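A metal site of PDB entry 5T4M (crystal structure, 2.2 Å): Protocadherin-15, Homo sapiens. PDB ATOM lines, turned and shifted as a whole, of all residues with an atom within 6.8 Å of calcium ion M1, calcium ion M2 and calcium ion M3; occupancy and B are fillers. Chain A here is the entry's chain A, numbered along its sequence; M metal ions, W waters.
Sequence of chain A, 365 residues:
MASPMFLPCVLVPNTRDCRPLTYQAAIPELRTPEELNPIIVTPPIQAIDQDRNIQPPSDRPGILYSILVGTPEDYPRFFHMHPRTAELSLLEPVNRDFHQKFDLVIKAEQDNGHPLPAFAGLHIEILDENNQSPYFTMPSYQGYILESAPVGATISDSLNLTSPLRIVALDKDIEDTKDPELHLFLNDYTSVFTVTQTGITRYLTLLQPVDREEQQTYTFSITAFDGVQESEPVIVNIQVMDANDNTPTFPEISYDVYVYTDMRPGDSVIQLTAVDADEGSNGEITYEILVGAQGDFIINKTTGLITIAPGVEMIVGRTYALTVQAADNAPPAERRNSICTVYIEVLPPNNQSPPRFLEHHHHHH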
ATOM      1  N   GLU A 147       0.250 -19.041   3.164  1.00  0.00           N
ATOM      2  CA  GLU A 147       0.170 -20.271   3.956  1.00  0.00           C
ATOM      3  C   GLU A 147      -1.126 -20.377   4.763  1.00  0.00           C
ATOM      4  O   GLU A 147      -1.513 -21.469   5.184  1.00  0.00           O
ATOM      5  CB  GLU A 147       1.368 -20.375   4.906  1.00  0.00           C
ATOM      6  CG  GLU A 147       1.397 -19.354   6.036  1.00  0.00           C
ATOM      7  CD  GLU A 147       2.571 -19.575   6.975  1.00  0.00           C
ATOM      8  OE1 GLU A 147       3.291 -18.608   7.295  1.00  0.00           O
ATOM      9  OE2 GLU A 147       2.781 -20.739   7.396  1.00  0.00           O
ATOM     10  N   VAL A 210      -0.971 -25.644   3.394  1.00  0.00           N
ATOM     11  CA  VAL A 210       0.484 -25.663   3.403  1.00  0.00           C
ATOM     12  C   VAL A 210       1.018 -24.794   4.534  1.00  0.00           C
ATOM     13  O   VAL A 210       0.389 -23.820   4.940  1.00  0.00           O
ATOM     14  CB  VAL A 210       1.077 -25.181   2.053  1.00  0.00           C
ATOM     15  CG1 VAL A 210       0.861 -26.237   0.985  1.00  0.00           C
ATOM     16  CG2 VAL A 210       0.464 -23.855   1.642  1.00  0.00           C
ATOM     17  N   ASP A 211       2.192 -25.162   5.042  1.00  0.00           N
ATOM     18  CA  ASP A 211       2.804 -24.476   6.163  1.00  0.00           C
ATOM     19  C   ASP A 211       4.213 -24.037   5.775  1.00  0.00           C
ATOM     20  O   ASP A 211       5.108 -24.863   5.605  1.00  0.00           O
ATOM     21  CB  ASP A 211       2.835 -25.391   7.390  1.00  0.00           C
ATOM     22  CG  ASP A 211       3.509 -24.769   8.601  1.00  0.00           C
ATOM     23  OD1 ASP A 211       3.697 -23.532   8.629  1.00  0.00           O
ATOM     24  OD2 ASP A 211       3.856 -25.514   9.540  1.00  0.00           O
ATOM     25  N   ARG A 212       4.401 -22.718   5.633  1.00  0.00           N
ATOM     26  CA  ARG A 212       5.681 -22.175   5.207  1.00  0.00           C
ATOM     27  C   ARG A 212       6.810 -22.632   6.102  1.00  0.00           C
ATOM     28  O   ARG A 212       7.903 -22.948   5.627  1.00  0.00           O
ATOM     29  CB  ARG A 212       5.660 -20.646   5.170  1.00  0.00           C
ATOM     30  CG  ARG A 212       6.860 -20.056   4.433  1.00  0.00           C
ATOM     31  CD  ARG A 212       7.226 -18.667   4.915  1.00  0.00           C
ATOM     32  NE  ARG A 212       7.608 -18.669   6.320  1.00  0.00           N
ATOM     33  CZ  ARG A 212       8.835 -18.908   6.771  1.00  0.00           C
ATOM     34  NH1 ARG A 212       9.823 -19.154   5.914  1.00  0.00           N
ATOM     35  NH2 ARG A 212       9.079 -18.888   8.077  1.00  0.00           N
ATOM     36  N   GLU A 213       6.541 -22.682   7.408  1.00  0.00           N
ATOM     37  CA  GLU A 213       7.550 -23.103   8.382  1.00  0.00           C
ATOM     38  C   GLU A 213       7.946 -24.573   8.184  1.00  0.00           C
ATOM     39  O   GLU A 213       8.997 -25.013   8.649  1.00  0.00           O
ATOM     40  CB  GLU A 213       7.058 -22.863   9.810  1.00  0.00           C
ATOM     41  CG  GLU A 213       7.186 -21.418  10.298  1.00  0.00           C
ATOM     42  CD  GLU A 213       6.231 -20.456   9.608  1.00  0.00           C
ATOM     43  OE1 GLU A 213       5.010 -20.722   9.581  1.00  0.00           O
ATOM     44  OE2 GLU A 213       6.693 -19.416   9.095  1.00  0.00           O
ATOM     45  N   GLU A 214       7.087 -25.334   7.500  1.00  0.00           N
ATOM     46  CA  GLU A 214       7.351 -26.733   7.192  1.00  0.00           C
ATOM     47  C   GLU A 214       8.057 -26.882   5.842  1.00  0.00           C
ATOM     48  O   GLU A 214       9.065 -27.562   5.745  1.00  0.00           O
ATOM     49  CB  GLU A 214       6.044 -27.524   7.210  1.00  0.00           C
ATOM     50  CG  GLU A 214       6.203 -29.029   7.343  1.00  0.00           C
ATOM     51  CD  GLU A 214       4.876 -29.737   7.534  1.00  0.00           C
ATOM     52  OE1 GLU A 214       3.894 -29.370   6.856  1.00  0.00           O
ATOM     53  OE2 GLU A 214       4.811 -30.665   8.369  1.00  0.00           O
ATOM     54  N   MET A 241       3.911 -18.147   0.914  1.00  0.00           N
ATOM     55  CA  MET A 241       4.182 -16.861   1.555  1.00  0.00           C
ATOM     56  C   MET A 241       3.846 -16.856   3.040  1.00  0.00           C
ATOM     57  O   MET A 241       2.878 -17.496   3.478  1.00  0.00           O
ATOM     58  CB  MET A 241       3.418 -15.751   0.823  1.00  0.00           C
ATOM     59  CG  MET A 241       3.862 -15.570  -0.625  1.00  0.00           C
ATOM     60  SD  MET A 241       2.892 -14.351  -1.526  1.00  0.00           S
ATOM     61  CE  MET A 241       3.429 -12.832  -0.753  1.00  0.00           C
ATOM     62  N   ASP A 242       4.647 -16.137   3.807  1.00  0.00           N
ATOM     63  CA  ASP A 242       4.556 -16.157   5.267  1.00  0.00           C
ATOM     64  C   ASP A 242       3.325 -15.451   5.802  1.00  0.00           C
ATOM     65  O   ASP A 242       2.976 -14.352   5.370  1.00  0.00           O
ATOM     66  CB  ASP A 242       5.816 -15.527   5.876  1.00  0.00           C
ATOM     67  CG  ASP A 242       5.901 -15.730   7.381  1.00  0.00           C
ATOM     68  OD1 ASP A 242       5.616 -16.848   7.860  1.00  0.00           O
ATOM     69  OD2 ASP A 242       6.254 -14.763   8.090  1.00  0.00           O
ATOM     70  N   ALA A 243       2.645 -16.121   6.732  1.00  0.00           N
ATOM     71  CA  ALA A 243       1.673 -15.466   7.595  1.00  0.00           C
ATOM     72  C   ALA A 243       2.269 -15.400   8.986  1.00  0.00           C
ATOM     73  O   ALA A 243       3.040 -16.278   9.377  1.00  0.00           O
ATOM     74  CB  ALA A 243       0.359 -16.218   7.601  1.00  0.00           C
ATOM     75  N   ASN A 244       1.926 -14.365   9.743  1.00  0.00           N
ATOM     76  CA  ASN A 244       2.383 -14.300  11.129  1.00  0.00           C
ATOM     77  C   ASN A 244       1.547 -15.230  11.990  1.00  0.00           C
ATOM     78  O   ASN A 244       0.636 -14.786  12.696  1.00  0.00           O
ATOM     79  CB  ASN A 244       2.304 -12.862  11.666  1.00  0.00           C
ATOM     80  CG  ASN A 244       3.097 -12.691  12.945  1.00  0.00           C
ATOM     81  OD1 ASN A 244       4.187 -13.242  13.090  1.00  0.00           O
ATOM     82  ND2 ASN A 244       2.545 -11.946  13.898  1.00  0.00           N
ATOM     83  N   ASP A 245       1.855 -16.521  11.899  1.00  0.00           N
ATOM     84  CA  ASP A 245       1.103 -17.544  12.613  1.00  0.00           C
ATOM     85  C   ASP A 245       1.977 -18.258  13.635  1.00  0.00           C
ATOM     86  O   ASP A 245       1.655 -19.362  14.082  1.00  0.00           O
ATOM     87  CB  ASP A 245       0.459 -18.538  11.619  1.00  0.00           C
ATOM     88  CG  ASP A 245       1.468 -19.486  10.952  1.00  0.00           C
ATOM     89  OD1 ASP A 245       2.671 -19.170  10.807  1.00  0.00           O
ATOM     90  OD2 ASP A 245       1.021 -20.576  10.538  1.00  0.00           O
ATOM     91  N   ASN A 246       3.080 -17.618  14.007  1.00  0.00           N
ATOM     92  CA  ASN A 246       3.904 -18.060  15.130  1.00  0.00           C
ATOM     93  C   ASN A 246       4.145 -16.933  16.145  1.00  0.00           C
ATOM     94  O   ASN A 246       4.436 -15.805  15.782  1.00  0.00           O
ATOM     95  CB  ASN A 246       5.246 -18.596  14.640  1.00  0.00           C
ATOM     96  CG  ASN A 246       5.116 -19.960  14.007  1.00  0.00           C
ATOM     97  OD1 ASN A 246       5.346 -20.981  14.659  1.00  0.00           O
ATOM     98  ND2 ASN A 246       4.721 -19.998  12.731  1.00  0.00           N
ATOM     99  N   THR A 247       4.007 -17.286  17.418  1.00  0.00           N
ATOM    100  CA  THR A 247       4.132 -16.335  18.514  1.00  0.00           C
ATOM    101  C   THR A 247       5.520 -16.422  19.143  1.00  0.00           C
ATOM    102  O   THR A 247       6.030 -17.514  19.361  1.00  0.00           O
ATOM    103  CB  THR A 247       3.054 -16.599  19.593  1.00  0.00           C
ATOM    104  OG1 THR A 247       1.755 -16.340  19.049  1.00  0.00           O
ATOM    105  CG2 THR A 247       3.262 -15.739  20.835  1.00  0.00           C
ATOM    106  N   PRO A 248       6.149 -15.259  19.418  1.00  0.00           N
ATOM    107  CA  PRO A 248       7.432 -15.254  20.125  1.00  0.00           C
ATOM    108  C   PRO A 248       7.332 -16.034  21.433  1.00  0.00           C
ATOM    109  O   PRO A 248       6.461 -15.743  22.250  1.00  0.00           O
ATOM    110  CB  PRO A 248       7.686 -13.765  20.393  1.00  0.00           C
ATOM    111  CG  PRO A 248       6.935 -13.065  19.317  1.00  0.00           C
ATOM    112  CD  PRO A 248       5.709 -13.905  19.050  1.00  0.00           C
ATOM    113  N   ASP A 276      10.761 -17.178  17.410  1.00  0.00           N
ATOM    114  CA  ASP A 276       9.678 -16.940  16.463  1.00  0.00           C
ATOM    115  C   ASP A 276      10.109 -17.477  15.094  1.00  0.00           C
ATOM    116  O   ASP A 276      11.116 -17.037  14.544  1.00  0.00           O
ATOM    117  CB  ASP A 276       9.336 -15.449  16.393  1.00  0.00           C
ATOM    118  CG  ASP A 276       7.975 -15.180  15.756  1.00  0.00           C
ATOM    119  OD1 ASP A 276       7.698 -15.684  14.646  1.00  0.00           O
ATOM    120  OD2 ASP A 276       7.181 -14.451  16.385  1.00  0.00           O
ATOM    121  N   ALA A 277       9.361 -18.439  14.559  1.00  0.00           N
ATOM    122  CA  ALA A 277       9.764 -19.152  13.346  1.00  0.00           C
ATOM    123  C   ALA A 277       9.307 -18.456  12.066  1.00  0.00           C
ATOM    124  O   ALA A 277       9.636 -18.907  10.973  1.00  0.00           O
ATOM    125  CB  ALA A 277       9.229 -20.577  13.389  1.00  0.00           C
ATOM    126  N   ASP A 278       8.555 -17.376  12.201  1.00  0.00           N
ATOM    127  CA  ASP A 278       8.032 -16.672  11.037  1.00  0.00           C
ATOM    128  C   ASP A 278       9.152 -15.957  10.268  1.00  0.00           C
ATOM    129  O   ASP A 278      10.293 -15.885  10.737  1.00  0.00           O
ATOM    130  CB  ASP A 278       6.954 -15.673  11.457  1.00  0.00           C
ATOM    131  CG  ASP A 278       5.708 -16.356  11.968  1.00  0.00           C
ATOM    132  OD1 ASP A 278       5.312 -17.395  11.404  1.00  0.00           O
ATOM    133  OD2 ASP A 278       5.120 -15.861  12.955  1.00  0.00           O
ATOM    134  N   GLU A 279       8.810 -15.426   9.105  1.00  0.00           N
ATOM    135  CA  GLU A 279       9.805 -14.859   8.199  1.00  0.00           C
ATOM    136  C   GLU A 279       9.927 -13.345   8.361  1.00  0.00           C
ATOM    137  O   GLU A 279       8.939 -12.652   8.571  1.00  0.00           O
ATOM    138  CB  GLU A 279       9.443 -15.203   6.753  1.00  0.00           C
ATOM    139  CG  GLU A 279      10.537 -14.960   5.741  1.00  0.00           C
ATOM    140  CD  GLU A 279      10.148 -15.368   4.335  1.00  0.00           C
ATOM    141  OE1 GLU A 279      11.018 -15.846   3.582  1.00  0.00           O
ATOM    142  OE2 GLU A 279       8.950 -15.219   3.978  1.00  0.00           O
ATOM    143  N   SER A 281      10.188  -9.639   9.354  1.00  0.00           N
ATOM    144  CA  SER A 281       9.700  -8.853  10.479  1.00  0.00           C
ATOM    145  C   SER A 281       8.644  -9.616  11.282  1.00  0.00           C
ATOM    146  O   SER A 281       8.412  -9.302  12.455  1.00  0.00           O
ATOM    147  CB  SER A 281       9.128  -7.518   9.983  1.00  0.00           C
ATOM    148  OG  SER A 281       7.946  -7.708   9.226  1.00  0.00           O
ATOM    149  N   ASN A 282       8.021 -10.611  10.660  1.00  0.00           N
ATOM    150  CA  ASN A 282       7.081 -11.477  11.360  1.00  0.00           C
ATOM    151  C   ASN A 282       7.788 -12.348  12.397  1.00  0.00           C
ATOM    152  O   ASN A 282       7.184 -12.811  13.365  1.00  0.00           O
ATOM    153  CB  ASN A 282       6.302 -12.359  10.381  1.00  0.00           C
ATOM    154  CG  ASN A 282       5.258 -11.588   9.598  1.00  0.00           C
ATOM    155  OD1 ASN A 282       4.815 -10.522  10.010  1.00  0.00           O
ATOM    156  ND2 ASN A 282       4.838 -12.151   8.464  1.00  0.00           N
ATOM    157  N   GLY A 283       9.086 -12.563  12.184  1.00  0.00           N
ATOM    158  CA  GLY A 283       9.896 -13.322  13.111  1.00  0.00           C
ATOM    159  C   GLY A 283      10.834 -12.449  13.934  1.00  0.00           C
ATOM    160  O   GLY A 283      11.526 -12.942  14.833  1.00  0.00           O
ATOM    161  N   GLU A 284      10.868 -11.160  13.615  1.00  0.00           N
ATOM    162  CA  GLU A 284      11.735 -10.214  14.306  1.00  0.00           C
ATOM    163  C   GLU A 284      11.203  -9.881  15.699  1.00  0.00           C
ATOM    164  O   GLU A 284      10.122  -9.311  15.835  1.00  0.00           O
ATOM    165  CB  GLU A 284      11.874  -8.930  13.476  1.00  0.00           C
ATOM    166  CG  GLU A 284      12.816  -7.894  14.054  1.00  0.00           C
ATOM    167  CD  GLU A 284      12.855  -6.616  13.231  1.00  0.00           C
ATOM    168  OE1 GLU A 284      12.241  -6.593  12.136  1.00  0.00           O
ATOM    169  OE2 GLU A 284      13.496  -5.643  13.669  1.00  0.00           O
ATOM    170  N   ASP A 328       6.717  -9.782  18.214  1.00  0.00           N
ATOM    171  CA  ASP A 328       7.274  -9.723  16.864  1.00  0.00           C
ATOM    172  C   ASP A 328       6.956  -8.385  16.216  1.00  0.00           C
ATOM    173  O   ASP A 328       6.095  -7.644  16.699  1.00  0.00           O
ATOM    174  CB  ASP A 328       6.777 -10.893  15.990  1.00  0.00           C
ATOM    175  CG  ASP A 328       5.261 -11.039  15.974  1.00  0.00           C
ATOM    176  OD1 ASP A 328       4.536 -10.028  16.092  1.00  0.00           O
ATOM    177  OD2 ASP A 328       4.799 -12.191  15.823  1.00  0.00           O
ATOM    178  N   ASN A 329       7.658  -8.066  15.139  1.00  0.00           N
ATOM    179  CA  ASN A 329       7.496  -6.776  14.485  1.00  0.00           C
ATOM    180  C   ASN A 329       6.616  -6.842  13.237  1.00  0.00           C
ATOM    181  O   ASN A 329       6.900  -6.200  12.226  1.00  0.00           O
ATOM    182  CB  ASN A 329       8.864  -6.188  14.130  1.00  0.00           C
ATOM    183  CG  ASN A 329       9.489  -5.461  15.307  1.00  0.00           C
ATOM    184  OD1 ASN A 329      10.212  -6.062  16.108  1.00  0.00           O
ATOM    185  ND2 ASN A 329       9.216  -4.169  15.422  1.00  0.00           N
ATOM    186  N   ALA A 330       5.557  -7.632  13.337  1.00  0.00           N
ATOM    187  CA  ALA A 330       4.496  -7.594  12.346  1.00  0.00           C
ATOM    188  C   ALA A 330       3.703  -6.317  12.577  1.00  0.00           C
ATOM    189  O   ALA A 330       3.798  -5.715  13.635  1.00  0.00           O
ATOM    190  CB  ALA A 330       3.606  -8.826  12.474  1.00  0.00           C
ATOM    191  N   GLU A 334      -1.550  -7.669  13.292  1.00  0.00           N
ATOM    192  CA  GLU A 334      -1.196  -9.084  13.251  1.00  0.00           C
ATOM    193  C   GLU A 334      -0.132  -9.459  14.273  1.00  0.00           C
ATOM    194  O   GLU A 334       0.298 -10.612  14.338  1.00  0.00           O
ATOM    195  CB  GLU A 334      -0.710  -9.470  11.851  1.00  0.00           C
ATOM    196  CG  GLU A 334      -1.718  -9.226  10.736  1.00  0.00           C
ATOM    197  CD  GLU A 334      -1.326  -8.043   9.875  1.00  0.00           C
ATOM    198  OE1 GLU A 334      -1.570  -6.883  10.289  1.00  0.00           O
ATOM    199  OE2 GLU A 334      -0.772  -8.263   8.778  1.00  0.00           O
ATOM    200  N   ARG A 336       2.040 -10.538  17.412  1.00  0.00           N
ATOM    201  CA  ARG A 336       1.894 -11.547  18.454  1.00  0.00           C
ATOM    202  C   ARG A 336       2.945 -11.346  19.546  1.00  0.00           C
ATOM    203  O   ARG A 336       4.055 -10.902  19.269  1.00  0.00           O
ATOM    204  CB  ARG A 336       2.019 -12.952  17.874  1.00  0.00           C
ATOM    205  CG  ARG A 336       0.838 -13.396  17.044  1.00  0.00           C
ATOM    206  CD  ARG A 336       1.143 -14.685  16.305  1.00  0.00           C
ATOM    207  NE  ARG A 336      -0.048 -15.184  15.612  1.00  0.00           N
ATOM    208  CZ  ARG A 336      -0.801 -16.184  16.073  1.00  0.00           C
ATOM    209  NH1 ARG A 336      -0.470 -16.797  17.199  1.00  0.00           N
ATOM    210  NH2 ARG A 336      -1.873 -16.572  15.387  1.00  0.00           N
HETATM  211 CA    CA M   1       4.480 -18.242   9.386  1.00  0.00          CA
HETATM  212 CA    CA M   2       2.897 -21.571   9.557  1.00  0.00          CA
HETATM  213 CA    CA M   3       5.718 -14.236  14.591  1.00  0.00          CA
HETATM  214  O   HOH W   1       3.333 -22.388  11.846  1.00  0.00           O
HETATM  215  O   HOH W   2       1.147 -22.973   9.114  1.00  0.00           O
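The side-chain carboxylate (OE1) of Glu 213 sits close to the side-chain amide nitrogen (ND2) of Asn 246 (3.2 Å). The side-chain carboxylate of Asp 245 sits close to the side-chain amide nitrogen of Asn 246 (2.9 Å). OD2 of Asp 242 lies within hydrogen-bond range of ND2 of Asn 282, 3.0 Å away. OD1 of Asp 242 sits close to NE of Arg 212. OD2 of Asp 242 lies within hydrogen-bond range of N of Glu 279 (2.8 Å). The backbone carbonyl oxygen (O) of Asn 244 lies within hydrogen-bond range of the guanidinium group (NE) of Arg 336, at 3.0 Å. The side-chain amide nitrogen of Asn 244 sits at hydrogen-bond distance from the backbone carbonyl oxygen of Glu 334 (2.6 Å). OD1 of Asp 328 sits at hydrogen-bond distance from N of Arg 336 (2.9 Å).
Within 4 Å of calcium ion M1: Glu 147, Glu 213, Asp 242, Ala 243, Asp 245, Asn 246 and Asp 278. The nearest printed residue that does not touch calcium ion M1 is Arg 212 (4.4 Å).
Within 4 Å of calcium ion M2: Glu 147, Asp 211, Glu 213, Asp 245 and Asn 246. The nearest printed residue that does not touch calcium ion M2 is Arg 212 (4.4 Å).
Within 4 Å of calcium ion M3: Asn 244, Asn 246, Asp 276, Asp 278, Asn 282 and Asp 328. The nearest printed residue that does not touch calcium ion M3 is Gly 283 (4.5 Å).
Calcium ion M1 is bound by OD1 of Asp 278 (2.3 Å), OD1 of Asp 242 (2.4 Å), OE1 of Glu 147 (2.4 Å), O of Ala 243 (2.4 Å), OD1 of Asp 245 (2.5 Å), OE2 of Glu 213 (2.5 Å) and OE1 of Glu 213 (2.5 Å). Calcium ion M1 has seven donor atoms within binding distance.
Calcium ion M2 is bound by the side-chain carboxylate (OE1) of Glu 213 (2.3 Å), water W2 (2.3 Å), the side-chain carboxylate (OD1) of Asp 211 (2.3 Å), the side-chain carboxylate (OE2) of Glu 147 (2.3 Å), the side-chain carboxylate (OD2) of Asp 245 (2.3 Å), water W1 (2.5 Å) and the side-chain carboxylate (OD1) of Asp 245 (2.7 Å).
OD2 of Asp 276 binds calcium ion M3 (2.3 Å). Calcium ion M3 is bound by O of Asn 246, 2.4 Å away. Calcium ion M3 is bound by OD1 of Asn 244 (2.4 Å). Calcium ion M3 is bound by OD2 of Asp 278 (2.4 Å). Calcium ion M3 is bound by the backbone carbonyl oxygen (O) of Asn 282, 2.4 Å away. Calcium ion M3 is bound by OD1 of Asp 276, 2.5 Å away. Calcium ion M3 is bound by the side-chain carboxylate (OD2) of Asp 328.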
